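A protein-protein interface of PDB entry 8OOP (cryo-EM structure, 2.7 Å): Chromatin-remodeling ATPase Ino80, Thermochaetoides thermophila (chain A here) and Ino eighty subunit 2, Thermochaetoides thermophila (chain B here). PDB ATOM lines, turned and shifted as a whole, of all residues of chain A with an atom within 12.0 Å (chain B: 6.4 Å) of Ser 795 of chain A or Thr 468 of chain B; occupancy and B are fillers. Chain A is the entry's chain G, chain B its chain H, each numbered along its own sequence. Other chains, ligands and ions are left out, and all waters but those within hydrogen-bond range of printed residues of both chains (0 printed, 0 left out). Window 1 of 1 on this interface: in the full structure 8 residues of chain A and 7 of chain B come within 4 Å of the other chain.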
ATOM      1  N   PRO A 786      14.756  -5.660  24.916  1.00  0.00           N
ATOM      2  CA  PRO A 786      15.999  -6.399  25.182  1.00  0.00           C
ATOM      3  C   PRO A 786      17.225  -5.852  24.466  1.00  0.00           C
ATOM      4  O   PRO A 786      17.150  -5.340  23.347  1.00  0.00           O
ATOM      5  CB  PRO A 786      15.671  -7.813  24.684  1.00  0.00           C
ATOM      6  CG  PRO A 786      14.187  -7.908  24.759  1.00  0.00           C
ATOM      7  CD  PRO A 786      13.707  -6.537  24.376  1.00  0.00           C
ATOM      8  N   THR A 787      18.372  -5.987  25.134  1.00  0.00           N
ATOM      9  CA  THR A 787      19.671  -5.647  24.574  1.00  0.00           C
ATOM     10  C   THR A 787      20.185  -6.760  23.656  1.00  0.00           C
ATOM     11  O   THR A 787      19.709  -7.895  23.715  1.00  0.00           O
ATOM     12  CB  THR A 787      20.664  -5.383  25.701  1.00  0.00           C
ATOM     13  OG1 THR A 787      21.062  -6.624  26.291  1.00  0.00           O
ATOM     14  CG2 THR A 787      20.033  -4.504  26.772  1.00  0.00           C
ATOM     15  N   PRO A 788      21.169  -6.456  22.799  1.00  0.00           N
ATOM     16  CA  PRO A 788      21.684  -7.477  21.865  1.00  0.00           C
ATOM     17  C   PRO A 788      22.267  -8.732  22.502  1.00  0.00           C
ATOM     18  O   PRO A 788      22.084  -9.826  21.953  1.00  0.00           O
ATOM     19  CB  PRO A 788      22.752  -6.704  21.077  1.00  0.00           C
ATOM     20  CG  PRO A 788      22.268  -5.306  21.089  1.00  0.00           C
ATOM     21  CD  PRO A 788      21.707  -5.125  22.477  1.00  0.00           C
ATOM     22  N   SER A 789      22.974  -8.622  23.629  1.00  0.00           N
ATOM     23  CA  SER A 789      23.436  -9.830  24.305  1.00  0.00           C
ATOM     24  C   SER A 789      22.298 -10.637  24.908  1.00  0.00           C
ATOM     25  O   SER A 789      22.364 -11.872  24.931  1.00  0.00           O
ATOM     26  CB  SER A 789      24.439  -9.477  25.399  1.00  0.00           C
ATOM     27  OG  SER A 789      25.552  -8.770  24.884  1.00  0.00           O
ATOM     28  N   GLU A 790      21.246  -9.977  25.388  1.00  0.00           N
ATOM     29  CA  GLU A 790      20.085 -10.711  25.871  1.00  0.00           C
ATOM     30  C   GLU A 790      19.423 -11.504  24.752  1.00  0.00           C
ATOM     31  O   GLU A 790      18.966 -12.631  24.970  1.00  0.00           O
ATOM     32  CB  GLU A 790      19.093  -9.747  26.513  1.00  0.00           C
ATOM     33  CG  GLU A 790      19.604  -9.161  27.807  1.00  0.00           C
ATOM     34  CD  GLU A 790      18.704  -8.084  28.358  1.00  0.00           C
ATOM     35  OE1 GLU A 790      18.002  -7.426  27.564  1.00  0.00           O
ATOM     36  OE2 GLU A 790      18.710  -7.885  29.589  1.00  0.00           O
ATOM     37  N   ILE A 791      19.371 -10.938  23.546  1.00  0.00           N
ATOM     38  CA  ILE A 791      18.847 -11.676  22.400  1.00  0.00           C
ATOM     39  C   ILE A 791      19.740 -12.864  22.051  1.00  0.00           C
ATOM     40  O   ILE A 791      19.243 -13.948  21.718  1.00  0.00           O
ATOM     41  CB  ILE A 791      18.668 -10.724  21.204  1.00  0.00           C
ATOM     42  CG1 ILE A 791      17.613  -9.666  21.531  1.00  0.00           C
ATOM     43  CG2 ILE A 791      18.244 -11.494  19.966  1.00  0.00           C
ATOM     44  CD1 ILE A 791      17.647  -8.464  20.614  1.00  0.00           C
ATOM     45  N   LYS A 792      21.061 -12.690  22.119  1.00  0.00           N
ATOM     46  CA  LYS A 792      21.973 -13.819  21.928  1.00  0.00           C
ATOM     47  C   LYS A 792      21.823 -14.865  23.027  1.00  0.00           C
ATOM     48  O   LYS A 792      21.660 -16.056  22.746  1.00  0.00           O
ATOM     49  CB  LYS A 792      23.417 -13.325  21.848  1.00  0.00           C
ATOM     50  CG  LYS A 792      23.743 -12.616  20.549  1.00  0.00           C
ATOM     51  CD  LYS A 792      25.189 -12.167  20.503  1.00  0.00           C
ATOM     52  CE  LYS A 792      25.491 -11.484  19.182  1.00  0.00           C
ATOM     53  NZ  LYS A 792      26.917 -11.071  19.077  1.00  0.00           N
ATOM     54  N   GLU A 793      21.874 -14.432  24.287  1.00  0.00           N
ATOM     55  CA  GLU A 793      21.773 -15.358  25.413  1.00  0.00           C
ATOM     56  C   GLU A 793      20.429 -16.077  25.453  1.00  0.00           C
ATOM     57  O   GLU A 793      20.361 -17.241  25.863  1.00  0.00           O
ATOM     58  CB  GLU A 793      22.035 -14.609  26.719  1.00  0.00           C
ATOM     59  CG  GLU A 793      23.485 -14.171  26.869  1.00  0.00           C
ATOM     60  CD  GLU A 793      23.661 -12.988  27.800  1.00  0.00           C
ATOM     61  OE1 GLU A 793      22.749 -12.724  28.614  1.00  0.00           O
ATOM     62  OE2 GLU A 793      24.712 -12.319  27.711  1.00  0.00           O
ATOM     63  N   ALA A 794      19.354 -15.407  25.035  1.00  0.00           N
ATOM     64  CA  ALA A 794      18.064 -16.073  24.888  1.00  0.00           C
ATOM     65  C   ALA A 794      18.021 -17.034  23.702  1.00  0.00           C
ATOM     66  O   ALA A 794      17.297 -18.035  23.756  1.00  0.00           O
ATOM     67  CB  ALA A 794      16.950 -15.036  24.758  1.00  0.00           C
ATOM     68  N   SER A 795      18.771 -16.766  22.632  1.00  0.00           N
ATOM     69  CA  SER A 795      18.651 -17.580  21.427  1.00  0.00           C
ATOM     70  C   SER A 795      19.596 -18.777  21.362  1.00  0.00           C
ATOM     71  O   SER A 795      19.228 -19.800  20.772  1.00  0.00           O
ATOM     72  CB  SER A 795      18.883 -16.709  20.190  1.00  0.00           C
ATOM     73  OG  SER A 795      20.124 -16.030  20.268  1.00  0.00           O
ATOM     74  N   PHE A 796      20.797 -18.698  21.932  1.00  0.00           N
ATOM     75  CA  PHE A 796      21.743 -19.807  21.857  1.00  0.00           C
ATOM     76  C   PHE A 796      21.695 -20.771  23.037  1.00  0.00           C
ATOM     77  O   PHE A 796      22.374 -21.802  22.991  1.00  0.00           O
ATOM     78  CB  PHE A 796      23.169 -19.276  21.692  1.00  0.00           C
ATOM     79  CG  PHE A 796      23.409 -18.619  20.371  1.00  0.00           C
ATOM     80  CD1 PHE A 796      23.358 -19.360  19.205  1.00  0.00           C
ATOM     81  CD2 PHE A 796      23.671 -17.265  20.285  1.00  0.00           C
ATOM     82  CE1 PHE A 796      23.568 -18.767  17.980  1.00  0.00           C
ATOM     83  CE2 PHE A 796      23.883 -16.665  19.060  1.00  0.00           C
ATOM     84  CZ  PHE A 796      23.832 -17.420  17.905  1.00  0.00           C
ATOM     85  N   GLY A 797      20.929 -20.476  24.082  1.00  0.00           N
ATOM     86  CA  GLY A 797      20.872 -21.331  25.246  1.00  0.00           C
ATOM     87  C   GLY A 797      20.331 -22.722  24.971  1.00  0.00           C
ATOM     88  O   GLY A 797      19.683 -22.975  23.952  1.00  0.00           O
ATOM     89  N   PRO A 798      20.615 -23.664  25.876  1.00  0.00           N
ATOM     90  CA  PRO A 798      20.069 -25.019  25.715  1.00  0.00           C
ATOM     91  C   PRO A 798      18.578 -25.102  25.977  1.00  0.00           C
ATOM     92  O   PRO A 798      17.913 -25.991  25.431  1.00  0.00           O
ATOM     93  CB  PRO A 798      20.869 -25.836  26.738  1.00  0.00           C
ATOM     94  CG  PRO A 798      21.192 -24.848  27.813  1.00  0.00           C
ATOM     95  CD  PRO A 798      21.432 -23.539  27.095  1.00  0.00           C
ATOM     96  N   ARG A 799      18.036 -24.214  26.803  1.00  0.00           N
ATOM     97  CA  ARG A 799      16.616 -24.137  27.095  1.00  0.00           C
ATOM     98  C   ARG A 799      16.115 -22.717  26.875  1.00  0.00           C
ATOM     99  O   ARG A 799      16.890 -21.761  26.975  1.00  0.00           O
ATOM    100  CB  ARG A 799      16.333 -24.589  28.536  1.00  0.00           C
ATOM    101  CG  ARG A 799      16.551 -26.082  28.749  1.00  0.00           C
ATOM    102  CD  ARG A 799      16.274 -26.507  30.183  1.00  0.00           C
ATOM    103  NE  ARG A 799      16.545 -27.924  30.388  1.00  0.00           N
ATOM    104  CZ  ARG A 799      17.753 -28.440  30.577  1.00  0.00           C
ATOM    105  NH1 ARG A 799      18.833 -27.678  30.608  1.00  0.00           N
ATOM    106  NH2 ARG A 799      17.879 -29.755  30.742  1.00  0.00           N
ATOM    107  N   PRO A 800      14.827 -22.551  26.566  1.00  0.00           N
ATOM    108  CA  PRO A 800      14.261 -21.201  26.437  1.00  0.00           C
ATOM    109  C   PRO A 800      14.402 -20.392  27.718  1.00  0.00           C
ATOM    110  O   PRO A 800      14.532 -20.932  28.818  1.00  0.00           O
ATOM    111  CB  PRO A 800      12.786 -21.467  26.103  1.00  0.00           C
ATOM    112  CG  PRO A 800      12.767 -22.860  25.549  1.00  0.00           C
ATOM    113  CD  PRO A 800      13.810 -23.587  26.336  1.00  0.00           C
ATOM    114  N   VAL A 801      14.385 -19.067  27.558  1.00  0.00           N
ATOM    115  CA  VAL A 801      14.402 -18.152  28.696  1.00  0.00           C
ATOM    116  C   VAL A 801      13.602 -16.896  28.356  1.00  0.00           C
ATOM    117  O   VAL A 801      13.629 -16.414  27.221  1.00  0.00           O
ATOM    118  CB  VAL A 801      15.854 -17.817  29.104  1.00  0.00           C
ATOM    119  CG1 VAL A 801      16.594 -17.153  27.963  1.00  0.00           C
ATOM    120  CG2 VAL A 801      15.872 -16.943  30.349  1.00  0.00           C
ATOM    121  N   THR A 802      12.876 -16.386  29.351  1.00  0.00           N
ATOM    122  CA  THR A 802      12.055 -15.188  29.239  1.00  0.00           C
ATOM    123  C   THR A 802      12.876 -13.921  29.476  1.00  0.00           C
ATOM    124  O   THR A 802      13.921 -13.936  30.128  1.00  0.00           O
ATOM    125  CB  THR A 802      10.890 -15.232  30.227  1.00  0.00           C
ATOM    126  OG1 THR A 802      11.395 -15.436  31.553  1.00  0.00           O
ATOM    127  CG2 THR A 802       9.929 -16.356  29.875  1.00  0.00           C
ATOM    128  N   LEU A 803      12.370 -12.809  28.941  1.00  0.00           N
ATOM    129  CA  LEU A 803      13.030 -11.511  28.976  1.00  0.00           C
ATOM    130  C   LEU A 803      12.163 -10.526  29.754  1.00  0.00           C
ATOM    131  O   LEU A 803      10.940 -10.676  29.798  1.00  0.00           O
ATOM    132  CB  LEU A 803      13.263 -11.019  27.549  1.00  0.00           C
ATOM    133  CG  LEU A 803      14.196 -11.932  26.747  1.00  0.00           C
ATOM    134  CD1 LEU A 803      14.182 -11.580  25.272  1.00  0.00           C
ATOM    135  CD2 LEU A 803      15.613 -11.881  27.301  1.00  0.00           C
ATOM    136  N   PRO A 806       8.955  -8.882  27.142  1.00  0.00           N
ATOM    137  CA  PRO A 806       9.120  -9.816  26.023  1.00  0.00           C
ATOM    138  C   PRO A 806       9.418  -9.115  24.709  1.00  0.00           C
ATOM    139  O   PRO A 806       9.797  -9.785  23.739  1.00  0.00           O
ATOM    140  CB  PRO A 806       7.775 -10.555  25.981  1.00  0.00           C
ATOM    141  CG  PRO A 806       6.802  -9.600  26.586  1.00  0.00           C
ATOM    142  CD  PRO A 806       7.568  -8.831  27.630  1.00  0.00           C
ATOM    143  N   MET B 446      22.062 -16.303  13.948  1.00  0.00           N
ATOM    144  CA  MET B 446      20.824 -16.199  14.713  1.00  0.00           C
ATOM    145  C   MET B 446      19.534 -16.321  13.907  1.00  0.00           C
ATOM    146  O   MET B 446      18.462 -16.382  14.518  1.00  0.00           O
ATOM    147  CB  MET B 446      20.801 -14.877  15.493  1.00  0.00           C
ATOM    148  CG  MET B 446      21.737 -14.862  16.695  1.00  0.00           C
ATOM    149  SD  MET B 446      21.363 -13.567  17.895  1.00  0.00           S
ATOM    150  CE  MET B 446      21.790 -12.099  16.969  1.00  0.00           C
ATOM    151  N   GLU B 464      24.789 -23.286  13.895  1.00  0.00           N
ATOM    152  CA  GLU B 464      24.966 -22.617  15.181  1.00  0.00           C
ATOM    153  C   GLU B 464      23.730 -22.683  16.072  1.00  0.00           C
ATOM    154  O   GLU B 464      23.855 -22.506  17.288  1.00  0.00           O
ATOM    155  CB  GLU B 464      25.376 -21.157  14.975  1.00  0.00           C
ATOM    156  CG  GLU B 464      26.688 -20.982  14.237  1.00  0.00           C
ATOM    157  CD  GLU B 464      26.513 -20.919  12.739  1.00  0.00           C
ATOM    158  OE1 GLU B 464      25.455 -21.357  12.243  1.00  0.00           O
ATOM    159  OE2 GLU B 464      27.437 -20.437  12.053  1.00  0.00           O
ATOM    160  N   LEU B 465      22.547 -22.926  15.507  1.00  0.00           N
ATOM    161  CA  LEU B 465      21.331 -23.054  16.302  1.00  0.00           C
ATOM    162  C   LEU B 465      20.921 -24.491  16.587  1.00  0.00           C
ATOM    163  O   LEU B 465      20.203 -24.724  17.564  1.00  0.00           O
ATOM    164  CB  LEU B 465      20.166 -22.339  15.615  1.00  0.00           C
ATOM    165  CG  LEU B 465      20.219 -20.817  15.675  1.00  0.00           C
ATOM    166  CD1 LEU B 465      19.088 -20.237  14.856  1.00  0.00           C
ATOM    167  CD2 LEU B 465      20.160 -20.346  17.120  1.00  0.00           C
ATOM    168  N   LEU B 466      21.352 -25.451  15.777  1.00  0.00           N
ATOM    169  CA  LEU B 466      21.256 -26.845  16.183  1.00  0.00           C
ATOM    170  C   LEU B 466      22.087 -27.062  17.441  1.00  0.00           C
ATOM    171  O   LEU B 466      23.190 -26.528  17.576  1.00  0.00           O
ATOM    172  CB  LEU B 466      21.724 -27.763  15.057  1.00  0.00           C
ATOM    173  CG  LEU B 466      21.086 -27.514  13.690  1.00  0.00           C
ATOM    174  CD1 LEU B 466      21.506 -28.595  12.708  1.00  0.00           C
ATOM    175  CD2 LEU B 466      19.571 -27.460  13.819  1.00  0.00           C
ATOM    176  N   GLY B 467      21.548 -27.847  18.370  1.00  0.00           N
ATOM    177  CA  GLY B 467      22.135 -27.968  19.684  1.00  0.00           C
ATOM    178  C   GLY B 467      21.749 -26.872  20.654  1.00  0.00           C
ATOM    179  O   GLY B 467      22.257 -26.861  21.781  1.00  0.00           O
ATOM    180  N   THR B 468      20.898 -25.938  20.244  1.00  0.00           N
ATOM    181  CA  THR B 468      20.244 -24.994  21.138  1.00  0.00           C
ATOM    182  C   THR B 468      18.783 -25.405  21.306  1.00  0.00           C
ATOM    183  O   THR B 468      18.304 -26.348  20.670  1.00  0.00           O
ATOM    184  CB  THR B 468      20.362 -23.564  20.607  1.00  0.00           C
ATOM    185  OG1 THR B 468      19.428 -23.368  19.539  1.00  0.00           O
ATOM    186  CG2 THR B 468      21.771 -23.293  20.093  1.00  0.00           C
ATOM    187  N   HIS B 469      18.072 -24.687  22.178  1.00  0.00           N
ATOM    188  CA  HIS B 469      16.635 -24.902  22.318  1.00  0.00           C
ATOM    189  C   HIS B 469      15.885 -24.667  21.011  1.00  0.00           C
ATOM    190  O   HIS B 469      14.832 -25.273  20.786  1.00  0.00           O
ATOM    191  CB  HIS B 469      16.081 -24.017  23.436  1.00  0.00           C
ATOM    192  CG  HIS B 469      15.965 -22.570  23.070  1.00  0.00           C
ATOM    193  ND1 HIS B 469      14.951 -22.080  22.278  1.00  0.00           N
ATOM    194  CD2 HIS B 469      16.727 -21.505  23.406  1.00  0.00           C
ATOM    195  CE1 HIS B 469      15.106 -20.777  22.128  1.00  0.00           C
ATOM    196  NE2 HIS B 469      16.175 -20.403  22.804  1.00  0.00           N
ATOM    197  N   ALA B 470      16.402 -23.791  20.143  1.00  0.00           N
ATOM    198  CA  ALA B 470      15.761 -23.546  18.854  1.00  0.00           C
ATOM    199  C   ALA B 470      15.820 -24.762  17.934  1.00  0.00           C
ATOM    200  O   ALA B 470      14.955 -24.918  17.065  1.00  0.00           O
ATOM    201  CB  ALA B 470      16.400 -22.335  18.176  1.00  0.00           C
ATOM    202  N   GLY B 471      16.829 -25.620  18.098  1.00  0.00           N
ATOM    203  CA  GLY B 471      16.940 -26.835  17.309  1.00  0.00           C
ATOM    204  C   GLY B 471      15.920 -27.909  17.637  1.00  0.00           C
ATOM    205  O   GLY B 471      15.656 -28.770  16.791  1.00  0.00           O
ATOM    206  N   VAL B 472      15.341 -27.872  18.840  1.00  0.00           N
ATOM    207  CA  VAL B 472      14.473 -28.948  19.321  1.00  0.00           C
ATOM    208  C   VAL B 472      13.308 -29.202  18.370  1.00  0.00           C
ATOM    209  O   VAL B 472      12.988 -30.355  18.058  1.00  0.00           O
ATOM    210  CB  VAL B 472      13.972 -28.628  20.742  1.00  0.00           C
ATOM    211  CG1 VAL B 472      12.980 -29.680  21.211  1.00  0.00           C
ATOM    212  CG2 VAL B 472      15.145 -28.517  21.709  1.00  0.00           C
ATOM    213  N   ALA B 476      16.699 -31.480  16.722  1.00  0.00           N
ATOM    214  CA  ALA B 476      18.145 -31.309  16.805  1.00  0.00           C
ATOM    215  C   ALA B 476      18.494 -30.440  18.013  1.00  0.00           C
ATOM    216  O   ALA B 476      19.302 -29.512  17.931  1.00  0.00           O
ATOM    217  CB  ALA B 476      18.699 -30.717  15.511  1.00  0.00           C
ATOM    218  N   GLY B 477      17.895 -30.737  19.163  1.00  0.00           N
ATOM    219  CA  GLY B 477      18.186 -30.009  20.376  1.00  0.00           C
ATOM    220  C   GLY B 477      19.553 -30.311  20.957  1.00  0.00           C
ATOM    221  O   GLY B 477      20.406 -30.923  20.308  1.00  0.00           O
ATOM    222  N   PRO B 478      19.797 -29.864  22.200  1.00  0.00           N
ATOM    223  CA  PRO B 478      21.038 -30.126  22.937  1.00  0.00           C
ATOM    224  C   PRO B 478      21.387 -31.610  23.011  1.00  0.00           C
ATOM    225  O   PRO B 478      20.521 -32.405  23.377  1.00  0.00           O
ATOM    226  CB  PRO B 478      20.745 -29.564  24.335  1.00  0.00           C
ATOM    227  CG  PRO B 478      19.678 -28.546  24.121  1.00  0.00           C
ATOM    228  CD  PRO B 478      18.835 -29.095  23.005  1.00  0.00           C
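O of Ala 794 of chain A is in hydrogen-bond range of NE2 of His 469 of chain B, at 2.8 Å.
The side-chain sulfur (SD) of Met 446 of chain B sits at hydrogen-bond distance from the side-chain hydroxyl (OG) of Ser 795 of chain A.
O of Gly 797 of chain A is in hydrogen-bond range of N of His 469 of chain B, 2.9 Å away.
The backbone carbonyl oxygen of Ile 791 of chain A lies within hydrogen-bond range of the side-chain hydroxyl of Ser 795 of chain A (2.7 Å).
O of Lys 792 of chain A sits at hydrogen-bond distance from OG of Ser 795 of chain A (2.9 Å).
OG1 of Thr 468 of chain B lies within hydrogen-bond range of O of Leu 465 of chain B (2.5 Å).
OG1 of Thr 468 of chain B lies close to N of Ala 470 of chain B (3.1 Å).
Among the printed residues, pairs that only touch across the chains: Lys 792 of chain A with Met 446 of chain B (3.7 Å), Ser 795 of chain A with Leu 465 of chain B (3.8 Å), Ser 795 of chain A with Thr 468 of chain B (3.8 Å), Ser 795 of chain A with His 469 of chain B (3.7 Å), Phe 796 of chain A with Met 446 of chain B (3.5 Å), Phe 796 of chain A with Glu 464 of chain B (3.7 Å), Phe 796 of chain A with Leu 465 of chain B (3.9 Å), Phe 796 of chain A with Thr 468 of chain B (3.3 Å), Gly 797 of chain A with Thr 468 of chain B (3.5 Å), Pro 798 of chain A with His 469 of chain B (3.4 Å), Pro 798 of chain A with Pro 478 of chain B (3.4 Å), Arg 799 of chain A with His 469 of chain B (3.6 Å) and Pro 800 of chain A with His 469 of chain B (3.7 Å).
Ser 789 of chain A touches none of the printed residues of chain B.
Printed residues of chain B within 4 Å of Pro 798 of chain A: His 469 (3.4 Å) and Pro 478 (3.4 Å).
Of the printed residues of chain B, Arg 799 of chain A touches His 469.
Of the printed residues of chain A, Glu 464 of chain B touches Phe 796.
No residue of chain A comes within 4 Å of Gly 467 of chain B.
Thr 468 of chain B touches three residues of chain A.
His 469 of chain B touches just these residues of chain A: Ala 794, Ser 795, Gly 797, Pro 798, Arg 799 and Pro 800.
No residue of chain A comes within 4 Å of Ala 470 of chain B.
Gly 471 of chain B touches none of the printed residues of chain A.
Val 472 of chain B touches none of the printed residues of chain A.
No residue of chain A comes within 4 Å of Ala 476 of chain B.
No residue of chain A comes within 4 Å of Gly 477 of chain B.
Of chain A, only Pro 798 (3.4 Å) comes within 4 Å of Pro 478 of chain B.
The nearest residue of chain B that does not touch Ser 795 of chain A is Ala 470 of chain B (4.6 Å).
Of the 19 printed residues of chain A, 8 touch a printed residue of chain B.
Of the 13 printed residues of chain B, 6 touch a printed residue of chain A.
Hydrophobic or aromatic side chains of chain B within 4 Å of the printed part of chain A: Met 446, Leu 465, His 469 and Pro 478.
Among the printed residues, 16 pairs touch across the chains.
Among the printed residues, no Asp or Glu carboxylate lies within 4 Å of a Lys or Arg side-chain nitrogen of the other chain.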
